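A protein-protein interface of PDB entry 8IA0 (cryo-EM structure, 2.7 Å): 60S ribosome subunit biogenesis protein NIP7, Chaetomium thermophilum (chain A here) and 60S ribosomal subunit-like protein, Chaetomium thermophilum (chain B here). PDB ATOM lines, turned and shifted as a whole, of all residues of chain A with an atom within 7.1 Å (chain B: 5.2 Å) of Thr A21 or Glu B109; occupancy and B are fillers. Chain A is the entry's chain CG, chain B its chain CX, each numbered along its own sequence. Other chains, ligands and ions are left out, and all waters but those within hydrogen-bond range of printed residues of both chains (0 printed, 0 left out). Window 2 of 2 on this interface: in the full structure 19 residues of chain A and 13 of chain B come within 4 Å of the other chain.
Among the printed residues, merely in contact across the chains: Leu A13 with Val B108, Asp A14 with Val B108, Ala A17 with Val B108, Thr A21 with Glu B109, Leu A23 with Leu B105 and Lys A24 with Leu B105.
Of chain B, only Glu B109 (3.6 Å) comes within 4 Å of Thr A21.
Of the printed residues of chain B, Leu A23 touches Leu B105.
Of the printed residues of chain B, Leu A13 touches Val B108 (3.9 Å).
Printed residues of chain A within 4 Å of Val B108: Leu A13 (3.9 Å), Asp A14 (3.5 Å) and Ala A17 (3.7 Å).
Of the printed residues of chain B, Lys A24 touches Leu B105 (3.5 Å).
Tyr A96 touches none of the printed residues of chain B.
Tyr A19 touches none of the printed residues of chain B.
The nearest residue of chain A that does not touch Glu B109 is Leu A23 (4.3 Å).
The nearest printed residue of chain B that does not touch Leu A23 is Glu B109 (4.3 Å).
Hydrophobic or aromatic side chains of chain A that line the printed part of chain B: Ala A17 and Leu A23.
Printed residues of chain B that touch a printed residue of chain A: Leu B105, Val B108, Glu B109 and Lys B112.
Hydrophobic or aromatic side chains of chain B within 4 Å of the printed part of chain A: Leu B105 and Val B108.
Among the printed residues, 7 pairs touch across the chains.
The side-chain carboxylate (OD1) of Asp A14 lies within salt-bridge range of the side-chain amino group (NZ) of Lys B112 (2.6 Å).
The guanidinium group of Arg A95 lies within hydrogen-bond range of the backbone carbonyl oxygen of Ala A17, 2.8 Å away.
The backbone NH (N) of Thr A21 is in hydrogen-bond range of the backbone carbonyl oxygen (O) of Asn A93, 3.2 Å away.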
ATOM      1  N   LEU A  13      18.644  -6.671 -15.524  1.00  0.00           N
ATOM      2  CA  LEU A  13      19.046  -7.708 -14.581  1.00  0.00           C
ATOM      3  C   LEU A  13      19.707  -7.121 -13.341  1.00  0.00           C
ATOM      4  O   LEU A  13      19.621  -7.715 -12.260  1.00  0.00           O
ATOM      5  CB  LEU A  13      19.981  -8.705 -15.261  1.00  0.00           C
ATOM      6  CG  LEU A  13      19.366  -9.546 -16.380  1.00  0.00           C
ATOM      7  CD1 LEU A  13      20.424 -10.397 -17.062  1.00  0.00           C
ATOM      8  CD2 LEU A  13      18.249 -10.417 -15.842  1.00  0.00           C
ATOM      9  N   ASP A  14      20.372  -5.974 -13.474  1.00  0.00           N
ATOM     10  CA  ASP A  14      20.970  -5.329 -12.311  1.00  0.00           C
ATOM     11  C   ASP A  14      19.905  -4.938 -11.297  1.00  0.00           C
ATOM     12  O   ASP A  14      20.085  -5.115 -10.086  1.00  0.00           O
ATOM     13  CB  ASP A  14      21.775  -4.105 -12.745  1.00  0.00           C
ATOM     14  CG  ASP A  14      23.269  -4.332 -12.661  1.00  0.00           C
ATOM     15  OD1 ASP A  14      23.711  -5.056 -11.745  1.00  0.00           O
ATOM     16  OD2 ASP A  14      24.002  -3.787 -13.511  1.00  0.00           O
ATOM     17  N   LEU A  16      16.929  -6.368 -11.079  1.00  0.00           N
ATOM     18  CA  LEU A  16      16.376  -7.618 -10.574  1.00  0.00           C
ATOM     19  C   LEU A  16      17.293  -8.293  -9.563  1.00  0.00           C
ATOM     20  O   LEU A  16      16.800  -8.878  -8.594  1.00  0.00           O
ATOM     21  CB  LEU A  16      16.085  -8.575 -11.729  1.00  0.00           C
ATOM     22  CG  LEU A  16      14.891  -8.240 -12.620  1.00  0.00           C
ATOM     23  CD1 LEU A  16      14.831  -9.194 -13.798  1.00  0.00           C
ATOM     24  CD2 LEU A  16      13.602  -8.291 -11.824  1.00  0.00           C
ATOM     25  N   ALA A  17      18.609  -8.230  -9.767  1.00  0.00           N
ATOM     26  CA  ALA A  17      19.560  -8.790  -8.816  1.00  0.00           C
ATOM     27  C   ALA A  17      19.519  -8.088  -7.469  1.00  0.00           C
ATOM     28  O   ALA A  17      19.919  -8.676  -6.458  1.00  0.00           O
ATOM     29  CB  ALA A  17      20.979  -8.719  -9.381  1.00  0.00           C
ATOM     30  N   ASN A  18      19.050  -6.841  -7.436  1.00  0.00           N
ATOM     31  CA  ASN A  18      18.907  -6.129  -6.173  1.00  0.00           C
ATOM     32  C   ASN A  18      17.831  -6.776  -5.309  1.00  0.00           C
ATOM     33  O   ASN A  18      17.871  -6.670  -4.079  1.00  0.00           O
ATOM     34  CB  ASN A  18      18.584  -4.659  -6.465  1.00  0.00           C
ATOM     35  CG  ASN A  18      18.549  -3.783  -5.220  1.00  0.00           C
ATOM     36  OD1 ASN A  18      18.728  -4.246  -4.097  1.00  0.00           O
ATOM     37  ND2 ASN A  18      18.317  -2.493  -5.428  1.00  0.00           N
ATOM     38  N   TYR A  19      16.891  -7.489  -5.927  1.00  0.00           N
ATOM     39  CA  TYR A  19      15.728  -8.014  -5.228  1.00  0.00           C
ATOM     40  C   TYR A  19      15.676  -9.533  -5.144  1.00  0.00           C
ATOM     41  O   TYR A  19      15.039 -10.056  -4.224  1.00  0.00           O
ATOM     42  CB  TYR A  19      14.448  -7.511  -5.908  1.00  0.00           C
ATOM     43  CG  TYR A  19      14.222  -6.028  -5.755  1.00  0.00           C
ATOM     44  CD1 TYR A  19      13.694  -5.506  -4.588  1.00  0.00           C
ATOM     45  CD2 TYR A  19      14.558  -5.150  -6.773  1.00  0.00           C
ATOM     46  CE1 TYR A  19      13.490  -4.154  -4.446  1.00  0.00           C
ATOM     47  CE2 TYR A  19      14.362  -3.795  -6.637  1.00  0.00           C
ATOM     48  CZ  TYR A  19      13.829  -3.303  -5.473  1.00  0.00           C
ATOM     49  OH  TYR A  19      13.630  -1.951  -5.336  1.00  0.00           O
ATOM     50  N   MET A  20      16.314 -10.257  -6.063  1.00  0.00           N
ATOM     51  CA  MET A  20      16.170 -11.705  -6.123  1.00  0.00           C
ATOM     52  C   MET A  20      17.538 -12.371  -6.164  1.00  0.00           C
ATOM     53  O   MET A  20      18.561 -11.735  -6.423  1.00  0.00           O
ATOM     54  CB  MET A  20      15.337 -12.145  -7.330  1.00  0.00           C
ATOM     55  CG  MET A  20      14.109 -11.301  -7.584  1.00  0.00           C
ATOM     56  SD  MET A  20      13.158 -11.879  -8.998  1.00  0.00           S
ATOM     57  CE  MET A  20      14.422 -12.743  -9.915  1.00  0.00           C
ATOM     58  N   THR A  21      17.537 -13.681  -5.903  1.00  0.00           N
ATOM     59  CA  THR A  21      18.763 -14.457  -5.756  1.00  0.00           C
ATOM     60  C   THR A  21      19.105 -15.265  -7.002  1.00  0.00           C
ATOM     61  O   THR A  21      20.151 -15.049  -7.621  1.00  0.00           O
ATOM     62  CB  THR A  21      18.637 -15.405  -4.558  1.00  0.00           C
ATOM     63  OG1 THR A  21      17.869 -16.552  -4.942  1.00  0.00           O
ATOM     64  CG2 THR A  21      17.938 -14.717  -3.413  1.00  0.00           C
ATOM     65  N   ASP A  22      18.236 -16.196  -7.384  1.00  0.00           N
ATOM     66  CA  ASP A  22      18.544 -17.153  -8.447  1.00  0.00           C
ATOM     67  C   ASP A  22      17.945 -16.673  -9.768  1.00  0.00           C
ATOM     68  O   ASP A  22      16.890 -17.122 -10.217  1.00  0.00           O
ATOM     69  CB  ASP A  22      18.033 -18.541  -8.074  1.00  0.00           C
ATOM     70  CG  ASP A  22      18.844 -19.183  -6.969  1.00  0.00           C
ATOM     71  OD1 ASP A  22      20.029 -18.821  -6.813  1.00  0.00           O
ATOM     72  OD2 ASP A  22      18.297 -20.050  -6.257  1.00  0.00           O
ATOM     73  N   LEU A  23      18.653 -15.732 -10.394  1.00  0.00           N
ATOM     74  CA  LEU A  23      18.213 -15.229 -11.686  1.00  0.00           C
ATOM     75  C   LEU A  23      18.440 -16.235 -12.805  1.00  0.00           C
ATOM     76  O   LEU A  23      17.852 -16.088 -13.881  1.00  0.00           O
ATOM     77  CB  LEU A  23      18.922 -13.917 -12.010  1.00  0.00           C
ATOM     78  CG  LEU A  23      18.493 -12.672 -11.237  1.00  0.00           C
ATOM     79  CD1 LEU A  23      19.658 -11.716 -11.091  1.00  0.00           C
ATOM     80  CD2 LEU A  23      17.342 -11.994 -11.950  1.00  0.00           C
ATOM     81  N   LYS A  24      19.281 -17.246 -12.577  1.00  0.00           N
ATOM     82  CA  LYS A  24      19.421 -18.326 -13.549  1.00  0.00           C
ATOM     83  C   LYS A  24      18.108 -19.071 -13.738  1.00  0.00           C
ATOM     84  O   LYS A  24      17.789 -19.512 -14.848  1.00  0.00           O
ATOM     85  CB  LYS A  24      20.519 -19.291 -13.106  1.00  0.00           C
ATOM     86  CG  LYS A  24      21.889 -18.990 -13.676  1.00  0.00           C
ATOM     87  CD  LYS A  24      22.731 -20.256 -13.742  1.00  0.00           C
ATOM     88  CE  LYS A  24      22.266 -21.190 -14.849  1.00  0.00           C
ATOM     89  NZ  LYS A  24      21.723 -20.467 -16.028  1.00  0.00           N
ATOM     90  N   SER A  25      17.335 -19.224 -12.663  1.00  0.00           N
ATOM     91  CA  SER A  25      16.074 -19.949 -12.753  1.00  0.00           C
ATOM     92  C   SER A  25      15.074 -19.219 -13.640  1.00  0.00           C
ATOM     93  O   SER A  25      14.173 -19.843 -14.212  1.00  0.00           O
ATOM     94  CB  SER A  25      15.498 -20.161 -11.354  1.00  0.00           C
ATOM     95  OG  SER A  25      15.171 -18.924 -10.746  1.00  0.00           O
ATOM     96  N   LEU A  90       9.082 -11.114  -8.105  1.00  0.00           N
ATOM     97  CA  LEU A  90       9.991 -10.752  -7.023  1.00  0.00           C
ATOM     98  C   LEU A  90       9.809 -11.668  -5.820  1.00  0.00           C
ATOM     99  O   LEU A  90      10.787 -12.069  -5.180  1.00  0.00           O
ATOM    100  CB  LEU A  90       9.762  -9.295  -6.625  1.00  0.00           C
ATOM    101  CG  LEU A  90      10.470  -8.196  -7.425  1.00  0.00           C
ATOM    102  CD1 LEU A  90      10.668  -6.952  -6.571  1.00  0.00           C
ATOM    103  CD2 LEU A  90      11.781  -8.671  -8.009  1.00  0.00           C
ATOM    104  N   ASN A  93      11.502 -15.557  -5.683  1.00  0.00           N
ATOM    105  CA  ASN A  93      12.897 -15.762  -5.305  1.00  0.00           C
ATOM    106  C   ASN A  93      13.428 -14.553  -4.549  1.00  0.00           C
ATOM    107  O   ASN A  93      14.544 -14.085  -4.779  1.00  0.00           O
ATOM    108  CB  ASN A  93      13.754 -16.050  -6.533  1.00  0.00           C
ATOM    109  CG  ASN A  93      13.467 -17.409  -7.137  1.00  0.00           C
ATOM    110  OD1 ASN A  93      13.458 -18.423  -6.439  1.00  0.00           O
ATOM    111  ND2 ASN A  93      13.230 -17.437  -8.444  1.00  0.00           N
ATOM    112  N   ALA A  94      12.626 -14.030  -3.627  1.00  0.00           N
ATOM    113  CA  ALA A  94      13.022 -12.854  -2.866  1.00  0.00           C
ATOM    114  C   ALA A  94      14.208 -13.166  -1.962  1.00  0.00           C
ATOM    115  O   ALA A  94      14.277 -14.221  -1.329  1.00  0.00           O
ATOM    116  CB  ALA A  94      11.853 -12.340  -2.030  1.00  0.00           C
ATOM    117  N   ARG A  95      15.152 -12.227  -1.907  1.00  0.00           N
ATOM    118  CA  ARG A  95      16.349 -12.401  -1.093  1.00  0.00           C
ATOM    119  C   ARG A  95      16.094 -12.019   0.362  1.00  0.00           C
ATOM    120  O   ARG A  95      16.363 -12.805   1.274  1.00  0.00           O
ATOM    121  CB  ARG A  95      17.508 -11.583  -1.672  1.00  0.00           C
ATOM    122  CG  ARG A  95      18.874 -12.064  -1.216  1.00  0.00           C
ATOM    123  CD  ARG A  95      19.893 -10.948  -1.192  1.00  0.00           C
ATOM    124  NE  ARG A  95      20.711 -10.932  -2.398  1.00  0.00           N
ATOM    125  CZ  ARG A  95      20.420 -10.240  -3.490  1.00  0.00           C
ATOM    126  NH1 ARG A  95      19.342  -9.480  -3.559  1.00  0.00           N
ATOM    127  NH2 ARG A  95      21.233 -10.313  -4.539  1.00  0.00           N
ATOM    128  N   TYR A  96      15.576 -10.818   0.591  1.00  0.00           N
ATOM    129  CA  TYR A  96      15.253 -10.344   1.927  1.00  0.00           C
ATOM    130  C   TYR A  96      13.759 -10.067   2.021  1.00  0.00           C
ATOM    131  O   TYR A  96      13.170  -9.480   1.111  1.00  0.00           O
ATOM    132  CB  TYR A  96      16.047  -9.086   2.272  1.00  0.00           C
ATOM    133  CG  TYR A  96      17.544  -9.296   2.295  1.00  0.00           C
ATOM    134  CD1 TYR A  96      18.126 -10.184   3.185  1.00  0.00           C
ATOM    135  CD2 TYR A  96      18.376  -8.591   1.438  1.00  0.00           C
ATOM    136  CE1 TYR A  96      19.491 -10.374   3.213  1.00  0.00           C
ATOM    137  CE2 TYR A  96      19.742  -8.771   1.461  1.00  0.00           C
ATOM    138  CZ  TYR A  96      20.294  -9.665   2.349  1.00  0.00           C
ATOM    139  OH  TYR A  96      21.656  -9.852   2.376  1.00  0.00           O
ATOM    140  N   LEU B 105      24.371 -12.327 -17.135  1.00  0.00           N
ATOM    141  CA  LEU B 105      23.872 -12.623 -15.798  1.00  0.00           C
ATOM    142  C   LEU B 105      25.008 -12.953 -14.836  1.00  0.00           C
ATOM    143  O   LEU B 105      24.960 -12.573 -13.660  1.00  0.00           O
ATOM    144  CB  LEU B 105      22.871 -13.771 -15.866  1.00  0.00           C
ATOM    145  CG  LEU B 105      22.232 -14.097 -14.526  1.00  0.00           C
ATOM    146  CD1 LEU B 105      21.467 -12.876 -14.072  1.00  0.00           C
ATOM    147  CD2 LEU B 105      21.318 -15.297 -14.645  1.00  0.00           C
ATOM    148  N   ALA B 106      26.031 -13.666 -15.310  1.00  0.00           N
ATOM    149  CA  ALA B 106      27.141 -14.043 -14.439  1.00  0.00           C
ATOM    150  C   ALA B 106      27.902 -12.820 -13.944  1.00  0.00           C
ATOM    151  O   ALA B 106      28.294 -12.758 -12.773  1.00  0.00           O
ATOM    152  CB  ALA B 106      28.079 -15.001 -15.168  1.00  0.00           C
ATOM    153  N   MET B 107      28.132 -11.841 -14.821  1.00  0.00           N
ATOM    154  CA  MET B 107      28.800 -10.612 -14.403  1.00  0.00           C
ATOM    155  C   MET B 107      27.978  -9.862 -13.364  1.00  0.00           C
ATOM    156  O   MET B 107      28.526  -9.336 -12.390  1.00  0.00           O
ATOM    157  CB  MET B 107      29.060  -9.714 -15.611  1.00  0.00           C
ATOM    158  CG  MET B 107      29.502 -10.438 -16.864  1.00  0.00           C
ATOM    159  SD  MET B 107      31.239 -10.160 -17.230  1.00  0.00           S
ATOM    160  CE  MET B 107      31.101  -8.761 -18.340  1.00  0.00           C
ATOM    161  N   VAL B 108      26.662  -9.788 -13.569  1.00  0.00           N
ATOM    162  CA  VAL B 108      25.796  -9.066 -12.641  1.00  0.00           C
ATOM    163  C   VAL B 108      25.830  -9.721 -11.267  1.00  0.00           C
ATOM    164  O   VAL B 108      25.924  -9.045 -10.237  1.00  0.00           O
ATOM    165  CB  VAL B 108      24.363  -8.996 -13.198  1.00  0.00           C
ATOM    166  CG1 VAL B 108      23.398  -8.508 -12.134  1.00  0.00           C
ATOM    167  CG2 VAL B 108      24.313  -8.102 -14.421  1.00  0.00           C
ATOM    168  N   GLU B 109      25.751 -11.052 -11.232  1.00  0.00           N
ATOM    169  CA  GLU B 109      25.797 -11.765  -9.961  1.00  0.00           C
ATOM    170  C   GLU B 109      27.145 -11.588  -9.273  1.00  0.00           C
ATOM    171  O   GLU B 109      27.210 -11.445  -8.047  1.00  0.00           O
ATOM    172  CB  GLU B 109      25.493 -13.246 -10.178  1.00  0.00           C
ATOM    173  CG  GLU B 109      24.036 -13.614  -9.964  1.00  0.00           C
ATOM    174  CD  GLU B 109      23.708 -15.007 -10.458  1.00  0.00           C
ATOM    175  OE1 GLU B 109      24.268 -15.419 -11.496  1.00  0.00           O
ATOM    176  OE2 GLU B 109      22.890 -15.692  -9.809  1.00  0.00           O
ATOM    177  N   ALA B 110      28.234 -11.605 -10.045  1.00  0.00           N
ATOM    178  CA  ALA B 110      29.557 -11.416  -9.460  1.00  0.00           C
ATOM    179  C   ALA B 110      29.695 -10.033  -8.836  1.00  0.00           C
ATOM    180  O   ALA B 110      30.259  -9.889  -7.745  1.00  0.00           O
ATOM    181  CB  ALA B 110      30.635 -11.636 -10.520  1.00  0.00           C
ATOM    182  N   GLU B 111      29.188  -9.003  -9.516  1.00  0.00           N
ATOM    183  CA  GLU B 111      29.290  -7.646  -8.993  1.00  0.00           C
ATOM    184  C   GLU B 111      28.498  -7.484  -7.702  1.00  0.00           C
ATOM    185  O   GLU B 111      28.959  -6.827  -6.761  1.00  0.00           O
ATOM    186  CB  GLU B 111      28.810  -6.646 -10.044  1.00  0.00           C
ATOM    187  CG  GLU B 111      29.810  -5.549 -10.359  1.00  0.00           C
ATOM    188  CD  GLU B 111      29.351  -4.650 -11.489  1.00  0.00           C
ATOM    189  OE1 GLU B 111      28.391  -5.025 -12.195  1.00  0.00           O
ATOM    190  OE2 GLU B 111      29.951  -3.570 -11.673  1.00  0.00           O
ATOM    191  N   LYS B 112      27.301  -8.067  -7.643  1.00  0.00           N
ATOM    192  CA  LYS B 112      26.474  -7.939  -6.448  1.00  0.00           C
ATOM    193  C   LYS B 112      27.101  -8.653  -5.257  1.00  0.00           C
ATOM    194  O   LYS B 112      27.059  -8.144  -4.131  1.00  0.00           O
ATOM    195  CB  LYS B 112      25.072  -8.480  -6.721  1.00  0.00           C
ATOM    196  CG  LYS B 112      23.991  -7.412  -6.737  1.00  0.00           C
ATOM    197  CD  LYS B 112      24.318  -6.309  -7.731  1.00  0.00           C
ATOM    198  CE  LYS B 112      23.147  -5.362  -7.908  1.00  0.00           C
ATOM    199  NZ  LYS B 112      23.208  -4.646  -9.210  1.00  0.00           N
ATOM    200  N   GLN B 113      27.679  -9.834  -5.483  1.00  0.00           N
ATOM    201  CA  GLN B 113      28.291 -10.585  -4.391  1.00  0.00           C
ATOM    202  C   GLN B 113      29.460  -9.816  -3.788  1.00  0.00           C
ATOM    203  O   GLN B 113      29.622  -9.766  -2.564  1.00  0.00           O
ATOM    204  CB  GLN B 113      28.744 -11.955  -4.891  1.00  0.00           C
ATOM    205  CG  GLN B 113      29.171 -12.903  -3.793  1.00  0.00           C
ATOM    206  CD  GLN B 113      28.634 -14.303  -4.000  1.00  0.00           C
ATOM    207  OE1 GLN B 113      27.949 -14.852  -3.137  1.00  0.00           O
ATOM    208  NE2 GLN B 113      28.941 -14.889  -5.149  1.00  0.00           N
ATOM    209  N   GLY B 114      30.286  -9.212  -4.635  1.00  0.00           N
ATOM    210  CA  GLY B 114      31.354  -8.353  -4.167  1.00  0.00           C
ATOM    211  C   GLY B 114      32.573  -9.079  -3.641  1.00  0.00           C
ATOM    212  O   GLY B 114      33.236  -9.814  -4.380  1.00  0.00           O
